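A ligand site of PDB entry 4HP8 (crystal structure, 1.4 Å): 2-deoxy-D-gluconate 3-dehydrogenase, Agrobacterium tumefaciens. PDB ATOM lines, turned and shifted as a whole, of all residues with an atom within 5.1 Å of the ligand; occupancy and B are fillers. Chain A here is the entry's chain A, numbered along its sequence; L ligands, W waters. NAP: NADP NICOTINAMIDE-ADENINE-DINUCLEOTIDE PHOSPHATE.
N of Ala 66 sits close to N6A of the ligand (3.3 Å).
Residues that only touch the ligand: Ala 138 (3.2 Å), Thr 190 (3.2 Å), Asn 189 (3.2 Å), Gly 20 (3.3 Å), Ala 87 (3.3 Å), Ile 89 (3.4 Å), Ile 63 (3.4 Å), Asn 188 (3.4 Å), Thr 19 (3.4 Å), Ile 137 (3.5 Å), Pro 182 (3.7 Å), Tyr 184 (3.7 Å), Val 109 (3.7 Å) and Ser 139 (3.9 Å).
Hydrophobic or aromatic side chains within 4 Å of the ligand: Leu 21, Phe 65, Ala 87, Ile 89, Val 109, Ile 137, Tyr 152, Pro 182 and Ile 185.
29 residues have an atom within 4 Å of the ligand: Gly 16, Asn 18, Thr 19, Gly 20, Leu 21, Arg 41, Arg 42, Ile 63, Asp 64, Phe 65, Ala 66, Asn 86, Ala 87, Gly 88, Ile 89, Val 109, Ile 137, Ala 138, Ser 139, Tyr 152, Lys 156, Pro 182, Gly 183, Tyr 184, Ile 185, Thr 187, Asn 188, Asn 189 and Thr 190.
The nearest printed residue that does not touch the ligand is Ala 17 (4.2 Å).
The backbone carbonyl oxygen (O) of Thr 187 is in hydrogen-bond range of the side-chain hydroxyl (OG1) of Thr 190.
The side-chain hydroxyl (OG1) of Thr 187 sits at hydrogen-bond distance from the backbone NH (N) of Asn 189 (3.1 Å).
The side-chain amide nitrogen (ND2) of Asn 18 lies close to the guanidinium group (NE) of Arg 42, 3.4 Å away.
The side-chain amide nitrogen (ND2) of Asn 86 is in hydrogen-bond range of the backbone carbonyl oxygen (O) of Gly 16 (3.2 Å).
ND2 of Asn 86 lies close to N of Gly 22 (3.3 Å).
The backbone NH of Ala 66 sits at hydrogen-bond distance from the side-chain carboxylate of Asp 64 (2.9 Å).
N of Ile 89 sits at hydrogen-bond distance from OD1 of Asn 110 (2.9 Å).
N of Leu 140 sits at hydrogen-bond distance from O of Pro 182 (3.4 Å).
OG1 of Thr 187 lies within hydrogen-bond range of O2N of the ligand (2.6 Å).
An oxygen (O3B) of the ligand sits at hydrogen-bond distance from the side-chain amide oxygen of Asn 18, at 2.7 Å.
The side-chain hydroxyl (OH) of Tyr 152 lies within hydrogen-bond range of an oxygen (O2D) of the ligand (2.7 Å).
The guanidinium group (NH2) of Arg 41 is in salt-bridge range of an oxygen (O2X) of the ligand (2.8 Å).
O of Asn 86 is in hydrogen-bond range of O3D of the ligand (2.8 Å).
The guanidinium group (NH2) of Arg 42 lies within salt-bridge range of an oxygen (O3X) of the ligand.
An oxygen (O1N) of the ligand is in hydrogen-bond range of the backbone NH (N) of Leu 21, 2.9 Å away.
N7N of the ligand sits at hydrogen-bond distance from O of Ile 185 (3.4 Å).
N1A of the ligand lies within hydrogen-bond range of N of Phe 65 (2.9 Å).
An oxygen (O3D) of the ligand sits at hydrogen-bond distance from the side-chain amino group (NZ) of Lys 156 (2.9 Å).
N6A of the ligand is in hydrogen-bond range of OD1 of Asp 64.
The backbone carbonyl oxygen (O) of Gly 16 lies close to an oxygen (O3B) of the ligand (3.2 Å).
A nitrogen (N7N) of the ligand sits close to the backbone carbonyl oxygen (O) of Gly 183 (3.2 Å).
The backbone NH (N) of Gly 88 lies within hydrogen-bond range of an oxygen (O4B) of the ligand (3.3 Å).
Water W11 bridges O2A of the ligand (2.8 Å) and ND2 of Asn 188 (2.9 Å).
Water W12 lies within hydrogen-bond range of an oxygen (O1A) of the ligand (2.8 Å), the backbone carbonyl oxygen of Asn 188 (3.3 Å) and the backbone NH of Asn 189 (3.4 Å).
Water W7 lies within hydrogen-bond range of the backbone NH (N) of Arg 41, an oxygen (O1X) of the ligand, the side-chain amide oxygen (OD1) of Asn 18 and the backbone NH (N) of Arg 42.
Water W4 bridges the backbone NH of Gly 16 and a nitrogen (N3A) of the ligand.
Water W10 lies within hydrogen-bond range of O of Pro 182, N of Leu 140, OG of Ser 139 and O of Gly 183.
Water W2 lies within hydrogen-bond range of O of Ala 87, O3D of the ligand, O of Asn 86 and NZ of Lys 156.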
ATOM      1  N   GLY A  16     -21.229  -1.378 -31.290  1.00  0.00           N
ATOM      2  CA  GLY A  16     -21.631  -2.769 -31.221  1.00  0.00           C
ATOM      3  C   GLY A  16     -22.834  -3.064 -32.074  1.00  0.00           C
ATOM      4  O   GLY A  16     -23.696  -3.836 -31.683  1.00  0.00           O
ATOM      5  N   ALA A  17     -22.911  -2.477 -33.270  1.00  0.00           N
ATOM      6  CA  ALA A  17     -24.164  -2.464 -34.014  1.00  0.00           C
ATOM      7  C   ALA A  17     -24.343  -3.641 -34.942  1.00  0.00           C
ATOM      8  O   ALA A  17     -25.375  -3.756 -35.591  1.00  0.00           O
ATOM      9  CB  ALA A  17     -24.263  -1.184 -34.824  1.00  0.00           C
ATOM     10  N   ASN A  18     -23.335  -4.518 -35.036  1.00  0.00           N
ATOM     11  CA  ASN A  18     -23.407  -5.676 -35.939  1.00  0.00           C
ATOM     12  C   ASN A  18     -24.287  -6.840 -35.451  1.00  0.00           C
ATOM     13  O   ASN A  18     -24.680  -7.689 -36.268  1.00  0.00           O
ATOM     14  CB  ASN A  18     -21.989  -6.193 -36.244  1.00  0.00           C
ATOM     15  CG  ASN A  18     -21.287  -6.663 -35.003  1.00  0.00           C
ATOM     16  OD1 ASN A  18     -21.041  -5.848 -34.128  1.00  0.00           O
ATOM     17  ND2 ASN A  18     -20.956  -7.945 -34.878  1.00  0.00           N
ATOM     18  N   THR A  19     -24.601  -6.890 -34.156  1.00  0.00           N
ATOM     19  CA  THR A  19     -25.328  -8.048 -33.628  1.00  0.00           C
ATOM     20  C   THR A  19     -26.026  -7.642 -32.340  1.00  0.00           C
ATOM     21  O   THR A  19     -25.817  -6.532 -31.826  1.00  0.00           O
ATOM     22  CB  THR A  19     -24.315  -9.171 -33.363  1.00  0.00           C
ATOM     23  OG1 THR A  19     -25.001 -10.377 -33.055  1.00  0.00           O
ATOM     24  CG2 THR A  19     -23.396  -8.805 -32.229  1.00  0.00           C
ATOM     25  N   GLY A  20     -26.858  -8.543 -31.826  1.00  0.00           N
ATOM     26  CA  GLY A  20     -27.340  -8.388 -30.443  1.00  0.00           C
ATOM     27  C   GLY A  20     -28.142  -7.120 -30.223  1.00  0.00           C
ATOM     28  O   GLY A  20     -28.919  -6.651 -31.054  1.00  0.00           O
ATOM     29  N   LEU A  21     -27.928  -6.557 -29.036  1.00  0.00           N
ATOM     30  CA  LEU A  21     -28.673  -5.332 -28.665  1.00  0.00           C
ATOM     31  C   LEU A  21     -28.359  -4.166 -29.570  1.00  0.00           C
ATOM     32  O   LEU A  21     -29.255  -3.409 -29.913  1.00  0.00           O
ATOM     33  CB  LEU A  21     -28.374  -4.899 -27.208  1.00  0.00           C
ATOM     34  CG  LEU A  21     -28.603  -6.007 -26.151  1.00  0.00           C
ATOM     35  CD1 LEU A  21     -28.598  -5.328 -24.757  1.00  0.00           C
ATOM     36  CD2 LEU A  21     -29.866  -6.835 -26.317  1.00  0.00           C
ATOM     37  N   GLY A  22     -27.086  -4.002 -29.963  1.00  0.00           N
ATOM     38  CA  GLY A  22     -26.745  -2.870 -30.810  1.00  0.00           C
ATOM     39  C   GLY A  22     -27.457  -2.960 -32.161  1.00  0.00           C
ATOM     40  O   GLY A  22     -27.905  -1.930 -32.678  1.00  0.00           O
ATOM     41  N   ALA A  40     -18.918  -0.796 -35.482  1.00  0.00           N
ATOM     42  CA  ALA A  40     -18.634  -2.166 -35.156  1.00  0.00           C
ATOM     43  C   ALA A  40     -17.181  -2.422 -35.479  1.00  0.00           C
ATOM     44  O   ALA A  40     -16.590  -1.687 -36.259  1.00  0.00           O
ATOM     45  CB  ALA A  40     -19.525  -3.085 -35.970  1.00  0.00           C
ATOM     46  N   ARG A  41     -16.608  -3.483 -34.928  1.00  0.00           N
ATOM     47  CA  ARG A  41     -15.232  -3.830 -35.318  1.00  0.00           C
ATOM     48  C   ARG A  41     -15.200  -4.748 -36.517  1.00  0.00           C
ATOM     49  O   ARG A  41     -14.107  -5.082 -37.038  1.00  0.00           O
ATOM     50  CB  ARG A  41     -14.429  -4.394 -34.122  1.00  0.00           C
ATOM     51  CG  ARG A  41     -15.083  -5.564 -33.443  1.00  0.00           C
ATOM     52  CD  ARG A  41     -14.188  -6.178 -32.358  1.00  0.00           C
ATOM     53  NE  ARG A  41     -14.919  -7.177 -31.612  1.00  0.00           N
ATOM     54  CZ  ARG A  41     -14.514  -7.735 -30.473  1.00  0.00           C
ATOM     55  NH1 ARG A  41     -13.352  -7.368 -29.920  1.00  0.00           N
ATOM     56  NH2 ARG A  41     -15.296  -8.604 -29.860  1.00  0.00           N
ATOM     57  N   ARG A  42     -16.360  -5.237 -36.957  1.00  0.00           N
ATOM     58  CA  ARG A  42     -16.424  -5.951 -38.227  1.00  0.00           C
ATOM     59  C   ARG A  42     -17.640  -5.465 -38.972  1.00  0.00           C
ATOM     60  O   ARG A  42     -18.560  -4.914 -38.363  1.00  0.00           O
ATOM     61  CB  ARG A  42     -16.479  -7.444 -38.002  1.00  0.00           C
ATOM     62  CG  ARG A  42     -17.520  -7.897 -37.041  1.00  0.00           C
ATOM     63  CD  ARG A  42     -17.277  -9.375 -36.640  1.00  0.00           C
ATOM     64  NE  ARG A  42     -18.122  -9.743 -35.497  1.00  0.00           N
ATOM     65  CZ  ARG A  42     -18.820 -10.875 -35.413  1.00  0.00           C
ATOM     66  NH1 ARG A  42     -18.782 -11.789 -36.390  1.00  0.00           N
ATOM     67  NH2 ARG A  42     -19.558 -11.125 -34.320  1.00  0.00           N
ATOM     68  N   ILE A  63     -14.650   0.498 -36.129  1.00  0.00           N
ATOM     69  CA  ILE A  63     -13.924   1.066 -35.005  1.00  0.00           C
ATOM     70  C   ILE A  63     -13.746  -0.029 -33.986  1.00  0.00           C
ATOM     71  O   ILE A  63     -14.619  -0.882 -33.771  1.00  0.00           O
ATOM     72  CB  ILE A  63     -14.664   2.262 -34.476  1.00  0.00           C
ATOM     73  CG1 ILE A  63     -13.867   2.961 -33.365  1.00  0.00           C
ATOM     74  CG2 ILE A  63     -16.093   1.897 -34.012  1.00  0.00           C
ATOM     75  CD1 ILE A  63     -14.445   4.362 -33.168  1.00  0.00           C
ATOM     76  N   ASP A  64     -12.573  -0.039 -33.376  1.00  0.00           N
ATOM     77  CA  ASP A  64     -12.201  -1.077 -32.417  1.00  0.00           C
ATOM     78  C   ASP A  64     -11.784  -0.413 -31.096  1.00  0.00           C
ATOM     79  O   ASP A  64     -10.733   0.220 -30.991  1.00  0.00           O
ATOM     80  CB  ASP A  64     -11.045  -1.966 -32.962  1.00  0.00           C
ATOM     81  CG  ASP A  64     -10.775  -3.151 -32.086  1.00  0.00           C
ATOM     82  OD1 ASP A  64     -11.049  -3.153 -30.905  1.00  0.00           O
ATOM     83  OD2 ASP A  64     -10.267  -4.197 -32.620  1.00  0.00           O
ATOM     84  N   PHE A  65     -12.631  -0.609 -30.103  1.00  0.00           N
ATOM     85  CA  PHE A  65     -12.454   0.033 -28.787  1.00  0.00           C
ATOM     86  C   PHE A  65     -11.448  -0.676 -27.886  1.00  0.00           C
ATOM     87  O   PHE A  65     -11.291  -0.282 -26.733  1.00  0.00           O
ATOM     88  CB  PHE A  65     -13.832   0.185 -28.092  1.00  0.00           C
ATOM     89  CG  PHE A  65     -14.718   1.166 -28.807  1.00  0.00           C
ATOM     90  CD1 PHE A  65     -14.378   2.527 -28.872  1.00  0.00           C
ATOM     91  CD2 PHE A  65     -15.824   0.739 -29.530  1.00  0.00           C
ATOM     92  CE1 PHE A  65     -15.170   3.447 -29.584  1.00  0.00           C
ATOM     93  CE2 PHE A  65     -16.618   1.663 -30.228  1.00  0.00           C
ATOM     94  CZ  PHE A  65     -16.301   3.001 -30.243  1.00  0.00           C
ATOM     95  N   ALA A  66     -10.755  -1.702 -28.382  1.00  0.00           N
ATOM     96  CA  ALA A  66      -9.566  -2.162 -27.662  1.00  0.00           C
ATOM     97  C   ALA A  66      -8.598  -0.990 -27.440  1.00  0.00           C
ATOM     98  O   ALA A  66      -7.858  -1.003 -26.426  1.00  0.00           O
ATOM     99  CB  ALA A  66      -8.891  -3.278 -28.414  1.00  0.00           C
ATOM    100  N   ASN A  86     -23.138   0.964 -26.690  1.00  0.00           N
ATOM    101  CA  ASN A  86     -23.550  -0.418 -26.513  1.00  0.00           C
ATOM    102  C   ASN A  86     -22.398  -1.421 -26.570  1.00  0.00           C
ATOM    103  O   ASN A  86     -22.541  -2.488 -25.971  1.00  0.00           O
ATOM    104  CB  ASN A  86     -24.613  -0.712 -27.562  1.00  0.00           C
ATOM    105  CG  ASN A  86     -24.938  -2.172 -27.680  1.00  0.00           C
ATOM    106  OD1 ASN A  86     -25.728  -2.747 -26.922  1.00  0.00           O
ATOM    107  ND2 ASN A  86     -24.310  -2.820 -28.669  1.00  0.00           N
ATOM    108  N   ALA A  87     -21.306  -1.134 -27.283  1.00  0.00           N
ATOM    109  CA  ALA A  87     -20.202  -2.101 -27.348  1.00  0.00           C
ATOM    110  C   ALA A  87     -19.755  -2.497 -25.943  1.00  0.00           C
ATOM    111  O   ALA A  87     -19.610  -1.641 -25.037  1.00  0.00           O
ATOM    112  CB  ALA A  87     -19.036  -1.536 -28.110  1.00  0.00           C
ATOM    113  N   GLY A  88     -19.506  -3.800 -25.759  1.00  0.00           N
ATOM    114  CA  GLY A  88     -19.121  -4.304 -24.423  1.00  0.00           C
ATOM    115  C   GLY A  88     -18.719  -5.725 -24.509  1.00  0.00           C
ATOM    116  O   GLY A  88     -19.159  -6.448 -25.435  1.00  0.00           O
ATOM    117  N   ILE A  89     -17.883  -6.168 -23.577  1.00  0.00           N
ATOM    118  CA  ILE A  89     -17.430  -7.562 -23.482  1.00  0.00           C
ATOM    119  C   ILE A  89     -17.544  -8.026 -22.043  1.00  0.00           C
ATOM    120  O   ILE A  89     -17.758  -7.234 -21.124  1.00  0.00           O
ATOM    121  CB  ILE A  89     -16.018  -7.756 -23.976  1.00  0.00           C
ATOM    122  CG1 ILE A  89     -15.024  -6.871 -23.189  1.00  0.00           C
ATOM    123  CG2 ILE A  89     -15.933  -7.471 -25.489  1.00  0.00           C
ATOM    124  CD1 ILE A  89     -13.579  -7.368 -23.423  1.00  0.00           C
ATOM    125  N   VAL A 109     -13.026  -1.566 -22.857  1.00  0.00           N
ATOM    126  CA  VAL A 109     -14.149  -1.456 -23.746  1.00  0.00           C
ATOM    127  C   VAL A 109     -15.396  -0.902 -23.016  1.00  0.00           C
ATOM    128  O   VAL A 109     -16.074  -0.008 -23.539  1.00  0.00           O
ATOM    129  CB  VAL A 109     -14.485  -2.830 -24.396  1.00  0.00           C
ATOM    130  CG1 VAL A 109     -15.735  -2.695 -25.274  1.00  0.00           C
ATOM    131  CG2 VAL A 109     -13.321  -3.332 -25.239  1.00  0.00           C
ATOM    132  N   ASN A 110     -15.681  -1.448 -21.854  1.00  0.00           N
ATOM    133  CA  ASN A 110     -16.999  -1.221 -21.252  1.00  0.00           C
ATOM    134  C   ASN A 110     -17.106   0.113 -20.521  1.00  0.00           C
ATOM    135  O   ASN A 110     -18.208   0.590 -20.275  1.00  0.00           O
ATOM    136  CB  ASN A 110     -17.305  -2.322 -20.240  1.00  0.00           C
ATOM    137  CG  ASN A 110     -17.529  -3.665 -20.906  1.00  0.00           C
ATOM    138  OD1 ASN A 110     -17.065  -3.941 -21.993  1.00  0.00           O
ATOM    139  ND2 ASN A 110     -18.213  -4.564 -20.187  1.00  0.00           N
ATOM    140  N   ILE A 137     -25.575   1.618 -22.376  1.00  0.00           N
ATOM    141  CA  ILE A 137     -26.144   0.317 -22.044  1.00  0.00           C
ATOM    142  C   ILE A 137     -25.448  -0.148 -20.768  1.00  0.00           C
ATOM    143  O   ILE A 137     -24.249  -0.482 -20.731  1.00  0.00           O
ATOM    144  CB  ILE A 137     -25.978  -0.705 -23.215  1.00  0.00           C
ATOM    145  CG1 ILE A 137     -26.582  -0.138 -24.507  1.00  0.00           C
ATOM    146  CG2 ILE A 137     -26.584  -2.037 -22.794  1.00  0.00           C
ATOM    147  CD1 ILE A 137     -28.092   0.288 -24.397  1.00  0.00           C
ATOM    148  N   ALA A 138     -26.241  -0.138 -19.700  1.00  0.00           N
ATOM    149  CA  ALA A 138     -25.837  -0.589 -18.378  1.00  0.00           C
ATOM    150  C   ALA A 138     -26.190  -2.093 -18.278  1.00  0.00           C
ATOM    151  O   ALA A 138     -26.076  -2.819 -19.262  1.00  0.00           O
ATOM    152  CB  ALA A 138     -26.520   0.261 -17.345  1.00  0.00           C
ATOM    153  N   SER A 139     -26.646  -2.590 -17.115  1.00  0.00           N
ATOM    154  CA  SER A 139     -26.833  -4.011 -16.908  1.00  0.00           C
ATOM    155  C   SER A 139     -27.578  -4.187 -15.578  1.00  0.00           C
ATOM    156  O   SER A 139     -27.552  -3.289 -14.710  1.00  0.00           O
ATOM    157  CB  SER A 139     -25.462  -4.697 -16.808  1.00  0.00           C
ATOM    158  OG  SER A 139     -25.564  -6.040 -16.403  1.00  0.00           O
ATOM    159  N   LEU A 140     -28.173  -5.361 -15.391  1.00  0.00           N
ATOM    160  CA  LEU A 140     -28.582  -5.708 -14.004  1.00  0.00           C
ATOM    161  C   LEU A 140     -27.376  -5.650 -13.056  1.00  0.00           C
ATOM    162  O   LEU A 140     -27.545  -5.400 -11.863  1.00  0.00           O
ATOM    163  CB  LEU A 140     -29.181  -7.106 -13.949  1.00  0.00           C
ATOM    164  CG  LEU A 140     -30.544  -7.222 -14.662  1.00  0.00           C
ATOM    165  CD1 LEU A 140     -30.853  -8.712 -14.762  1.00  0.00           C
ATOM    166  CD2 LEU A 140     -31.594  -6.453 -13.952  1.00  0.00           C
ATOM    167  N   TYR A 152     -16.647  -6.877 -15.162  1.00  0.00           N
ATOM    168  CA  TYR A 152     -17.874  -6.501 -15.808  1.00  0.00           C
ATOM    169  C   TYR A 152     -18.812  -5.769 -14.833  1.00  0.00           C
ATOM    170  O   TYR A 152     -19.350  -4.722 -15.132  1.00  0.00           O
ATOM    171  CB  TYR A 152     -18.555  -7.765 -16.320  1.00  0.00           C
ATOM    172  CG  TYR A 152     -19.807  -7.494 -17.136  1.00  0.00           C
ATOM    173  CD1 TYR A 152     -19.711  -7.185 -18.500  1.00  0.00           C
ATOM    174  CD2 TYR A 152     -21.077  -7.556 -16.537  1.00  0.00           C
ATOM    175  CE1 TYR A 152     -20.871  -6.980 -19.265  1.00  0.00           C
ATOM    176  CE2 TYR A 152     -22.225  -7.323 -17.296  1.00  0.00           C
ATOM    177  CZ  TYR A 152     -22.091  -7.060 -18.627  1.00  0.00           C
ATOM    178  OH  TYR A 152     -23.268  -6.858 -19.378  1.00  0.00           O
ATOM    179  N   LYS A 156     -19.947  -2.001 -15.217  1.00  0.00           N
ATOM    180  CA  LYS A 156     -21.338  -1.625 -15.424  1.00  0.00           C
ATOM    181  C   LYS A 156     -21.866  -0.765 -14.299  1.00  0.00           C
ATOM    182  O   LYS A 156     -22.683   0.123 -14.542  1.00  0.00           O
ATOM    183  CB  LYS A 156     -22.220  -2.859 -15.657  1.00  0.00           C
ATOM    184  CG  LYS A 156     -21.932  -3.564 -16.982  1.00  0.00           C
ATOM    185  CD  LYS A 156     -22.220  -2.673 -18.223  1.00  0.00           C
ATOM    186  CE  LYS A 156     -22.279  -3.533 -19.498  1.00  0.00           C
ATOM    187  NZ  LYS A 156     -22.409  -2.641 -20.674  1.00  0.00           N
ATOM    188  N   PRO A 182     -30.559  -3.551 -19.482  1.00  0.00           N
ATOM    189  CA  PRO A 182     -31.296  -4.743 -19.939  1.00  0.00           C
ATOM    190  C   PRO A 182     -31.221  -5.816 -18.875  1.00  0.00           C
ATOM    191  O   PRO A 182     -30.203  -5.868 -18.094  1.00  0.00           O
ATOM    192  CB  PRO A 182     -30.478  -5.216 -21.152  1.00  0.00           C
ATOM    193  CG  PRO A 182     -29.670  -4.012 -21.583  1.00  0.00           C
ATOM    194  CD  PRO A 182     -29.308  -3.378 -20.242  1.00  0.00           C
ATOM    195  N   GLY A 183     -32.229  -6.692 -18.820  1.00  0.00           N
ATOM    196  CA  GLY A 183     -32.192  -7.895 -18.016  1.00  0.00           C
ATOM    197  C   GLY A 183     -31.372  -8.944 -18.703  1.00  0.00           C
ATOM    198  O   GLY A 183     -30.366  -8.620 -19.367  1.00  0.00           O
ATOM    199  N   TYR A 184     -31.795 -10.183 -18.608  1.00  0.00           N
ATOM    200  CA  TYR A 184     -31.093 -11.287 -19.257  1.00  0.00           C
ATOM    201  C   TYR A 184     -31.735 -11.446 -20.619  1.00  0.00           C
ATOM    202  O   TYR A 184     -32.897 -11.784 -20.772  1.00  0.00           O
ATOM    203  CB  TYR A 184     -31.096 -12.553 -18.333  1.00  0.00           C
ATOM    204  CG  TYR A 184     -29.967 -12.426 -17.294  1.00  0.00           C
ATOM    205  CD1 TYR A 184     -30.219 -12.000 -15.999  1.00  0.00           C
ATOM    206  CD2 TYR A 184     -28.647 -12.742 -17.624  1.00  0.00           C
ATOM    207  CE1 TYR A 184     -29.173 -11.836 -15.066  1.00  0.00           C
ATOM    208  CE2 TYR A 184     -27.597 -12.598 -16.700  1.00  0.00           C
ATOM    209  CZ  TYR A 184     -27.872 -12.143 -15.438  1.00  0.00           C
ATOM    210  OH  TYR A 184     -26.829 -11.987 -14.511  1.00  0.00           O
ATOM    211  N   ILE A 185     -30.948 -11.145 -21.664  1.00  0.00           N
ATOM    212  CA  ILE A 185     -31.396 -11.121 -23.051  1.00  0.00           C
ATOM    213  C   ILE A 185     -30.620 -12.184 -23.826  1.00  0.00           C
ATOM    214  O   ILE A 185     -29.393 -12.336 -23.605  1.00  0.00           O
ATOM    215  CB  ILE A 185     -31.146  -9.719 -23.707  1.00  0.00           C
ATOM    216  CG1 ILE A 185     -31.490  -8.545 -22.768  1.00  0.00           C
ATOM    217  CG2 ILE A 185     -31.869  -9.641 -25.081  1.00  0.00           C
ATOM    218  CD1 ILE A 185     -32.964  -8.459 -22.343  1.00  0.00           C
ATOM    219  N   THR A 187     -28.416 -13.308 -26.410  1.00  0.00           N
ATOM    220  CA  THR A 187     -27.441 -12.782 -27.369  1.00  0.00           C
ATOM    221  C   THR A 187     -26.130 -13.527 -27.145  1.00  0.00           C
ATOM    222  O   THR A 187     -26.015 -14.357 -26.249  1.00  0.00           O
ATOM    223  CB  THR A 187     -27.097 -11.303 -27.099  1.00  0.00           C
ATOM    224  OG1 THR A 187     -26.322 -11.232 -25.908  1.00  0.00           O
ATOM    225  CG2 THR A 187     -28.353 -10.385 -26.986  1.00  0.00           C
ATOM    226  N   ASN A 188     -25.106 -13.204 -27.933  1.00  0.00           N
ATOM    227  CA  ASN A 188     -23.781 -13.826 -27.693  1.00  0.00           C
ATOM    228  C   ASN A 188     -23.218 -13.590 -26.273  1.00  0.00           C
ATOM    229  O   ASN A 188     -22.529 -14.447 -25.716  1.00  0.00           O
ATOM    230  CB  ASN A 188     -22.788 -13.314 -28.757  1.00  0.00           C
ATOM    231  CG  ASN A 188     -23.211 -13.687 -30.198  1.00  0.00           C
ATOM    232  OD1 ASN A 188     -24.025 -14.601 -30.406  1.00  0.00           O
ATOM    233  ND2 ASN A 188     -22.630 -12.988 -31.205  1.00  0.00           N
ATOM    234  N   ASN A 189     -23.533 -12.454 -25.676  1.00  0.00           N
ATOM    235  CA  ASN A 189     -23.042 -12.105 -24.334  1.00  0.00           C
ATOM    236  C   ASN A 189     -23.433 -13.168 -23.274  1.00  0.00           C
ATOM    237  O   ASN A 189     -22.700 -13.447 -22.327  1.00  0.00           O
ATOM    238  CB  ASN A 189     -23.589 -10.713 -23.946  1.00  0.00           C
ATOM    239  CG  ASN A 189     -23.269 -10.315 -22.507  1.00  0.00           C
ATOM    240  OD1 ASN A 189     -23.949 -10.748 -21.568  1.00  0.00           O
ATOM    241  ND2 ASN A 189     -22.264  -9.426 -22.328  1.00  0.00           N
ATOM    242  N   THR A 190     -24.600 -13.759 -23.476  1.00  0.00           N
ATOM    243  CA  THR A 190     -25.161 -14.660 -22.458  1.00  0.00           C
ATOM    244  C   THR A 190     -25.180 -16.106 -22.904  1.00  0.00           C
ATOM    245  O   THR A 190     -25.719 -16.975 -22.198  1.00  0.00           O
ATOM    246  CB  THR A 190     -26.607 -14.264 -22.103  1.00  0.00           C
ATOM    247  OG1 THR A 190     -27.413 -14.284 -23.297  1.00  0.00           O
ATOM    248  CG2 THR A 190     -26.658 -12.925 -21.451  1.00  0.00           C
HETATM  249  PA  NAP L   1     -22.630  -9.176 -27.837  1.00  0.00           P
HETATM  250  O1A NAP L   1     -21.424  -9.698 -27.126  1.00  0.00           O
HETATM  251  O2A NAP L   1     -23.065  -9.917 -29.010  1.00  0.00           O
HETATM  252  O5B NAP L   1     -22.465  -7.660 -28.276  1.00  0.00           O
HETATM  253  C5B NAP L   1     -21.334  -6.891 -27.924  1.00  0.00           C
HETATM  254  C4B NAP L   1     -21.137  -5.921 -29.097  1.00  0.00           C
HETATM  255  O4B NAP L   1     -20.002  -5.112 -28.772  1.00  0.00           O
HETATM  256  C3B NAP L   1     -20.777  -6.662 -30.368  1.00  0.00           C
HETATM  257  O3B NAP L   1     -21.243  -5.861 -31.447  1.00  0.00           O
HETATM  258  C2B NAP L   1     -19.263  -6.627 -30.271  1.00  0.00           C
HETATM  259  O2B NAP L   1     -18.595  -6.897 -31.522  1.00  0.00           O
HETATM  260  C1B NAP L   1     -19.007  -5.213 -29.773  1.00  0.00           C
HETATM  261  N9A NAP L   1     -17.666  -5.055 -29.268  1.00  0.00           N
HETATM  262  C8A NAP L   1     -17.036  -5.783 -28.280  1.00  0.00           C
HETATM  263  N7A NAP L   1     -15.743  -5.447 -28.197  1.00  0.00           N
HETATM  264  C5A NAP L   1     -15.544  -4.456 -29.095  1.00  0.00           C
HETATM  265  C6A NAP L   1     -14.422  -3.729 -29.465  1.00  0.00           C
HETATM  266  N6A NAP L   1     -13.206  -3.904 -28.912  1.00  0.00           N
HETATM  267  N1A NAP L   1     -14.550  -2.787 -30.448  1.00  0.00           N
HETATM  268  C2A NAP L   1     -15.775  -2.587 -31.054  1.00  0.00           C
HETATM  269  N3A NAP L   1     -16.895  -3.311 -30.730  1.00  0.00           N
HETATM  270  C4A NAP L   1     -16.749  -4.212 -29.780  1.00  0.00           C
HETATM  271  O3  NAP L   1     -23.790  -9.121 -26.768  1.00  0.00           O
HETATM  272  PN  NAP L   1     -24.949  -8.048 -26.488  1.00  0.00           P
HETATM  273  O1N NAP L   1     -25.614  -7.588 -27.715  1.00  0.00           O
HETATM  274  O2N NAP L   1     -25.810  -8.722 -25.459  1.00  0.00           O
HETATM  275  O5D NAP L   1     -24.113  -6.873 -25.810  1.00  0.00           O
HETATM  276  C5D NAP L   1     -24.420  -5.498 -26.073  1.00  0.00           C
HETATM  277  C4D NAP L   1     -24.328  -4.720 -24.783  1.00  0.00           C
HETATM  278  O4D NAP L   1     -25.390  -5.139 -23.902  1.00  0.00           O
HETATM  279  C3D NAP L   1     -23.014  -4.908 -23.995  1.00  0.00           C
HETATM  280  O3D NAP L   1     -22.552  -3.699 -23.410  1.00  0.00           O
HETATM  281  C2D NAP L   1     -23.443  -5.864 -22.927  1.00  0.00           C
HETATM  282  O2D NAP L   1     -22.626  -5.754 -21.781  1.00  0.00           O
HETATM  283  C1D NAP L   1     -24.822  -5.296 -22.627  1.00  0.00           C
HETATM  284  N1N NAP L   1     -25.717  -6.165 -21.876  1.00  0.00           N
HETATM  285  C2N NAP L   1     -26.129  -7.392 -22.325  1.00  0.00           C
HETATM  286  C3N NAP L   1     -27.003  -8.159 -21.588  1.00  0.00           C
HETATM  287  C7N NAP L   1     -27.556  -9.384 -22.117  1.00  0.00           C
HETATM  288  O7N NAP L   1     -27.426  -9.772 -23.442  1.00  0.00           O
HETATM  289  N7N NAP L   1     -28.253 -10.119 -21.279  1.00  0.00           N
HETATM  290  C4N NAP L   1     -27.475  -7.736 -20.340  1.00  0.00           C
HETATM  291  C5N NAP L   1     -27.092  -6.454 -19.939  1.00  0.00           C
HETATM  292  C6N NAP L   1     -26.242  -5.652 -20.696  1.00  0.00           C
HETATM  293  P2B NAP L   1     -18.356  -8.413 -32.045  1.00  0.00           P
HETATM  294  O1X NAP L   1     -17.352  -8.220 -33.121  1.00  0.00           O
HETATM  295  O2X NAP L   1     -17.839  -9.229 -30.876  1.00  0.00           O
HETATM  296  O3X NAP L   1     -19.670  -8.907 -32.526  1.00  0.00           O
HETATM  297  O   HOH W   1     -11.436  -5.678 -27.116  1.00  0.00           O
HETATM  298  O   HOH W   2     -21.795  -0.560 -23.343  1.00  0.00           O
HETATM  299  O   HOH W   3     -15.279  -9.859 -33.828  1.00  0.00           O
HETATM  300  O   HOH W   4     -18.447  -1.146 -31.826  1.00  0.00           O
HETATM  301  O   HOH W   5     -20.523  -8.856 -24.752  1.00  0.00           O
HETATM  302  O   HOH W   6     -25.224 -11.152 -30.066  1.00  0.00           O
HETATM  303  O   HOH W   7     -18.167  -5.767 -34.365  1.00  0.00           O
HETATM  304  O   HOH W   8     -24.690  -5.586 -29.355  1.00  0.00           O
HETATM  305  O   HOH W   9     -17.103 -11.761 -30.912  1.00  0.00           O
HETATM  306  O   HOH W  10     -28.249  -7.574 -17.202  1.00  0.00           O
HETATM  307  O   HOH W  11     -20.892 -10.720 -30.627  1.00  0.00           O
HETATM  308  O   HOH W  12     -20.403 -12.334 -26.988  1.00  0.00           O
HETATM  309  O   HOH W  13     -18.725  -9.369 -28.114  1.00  0.00           O
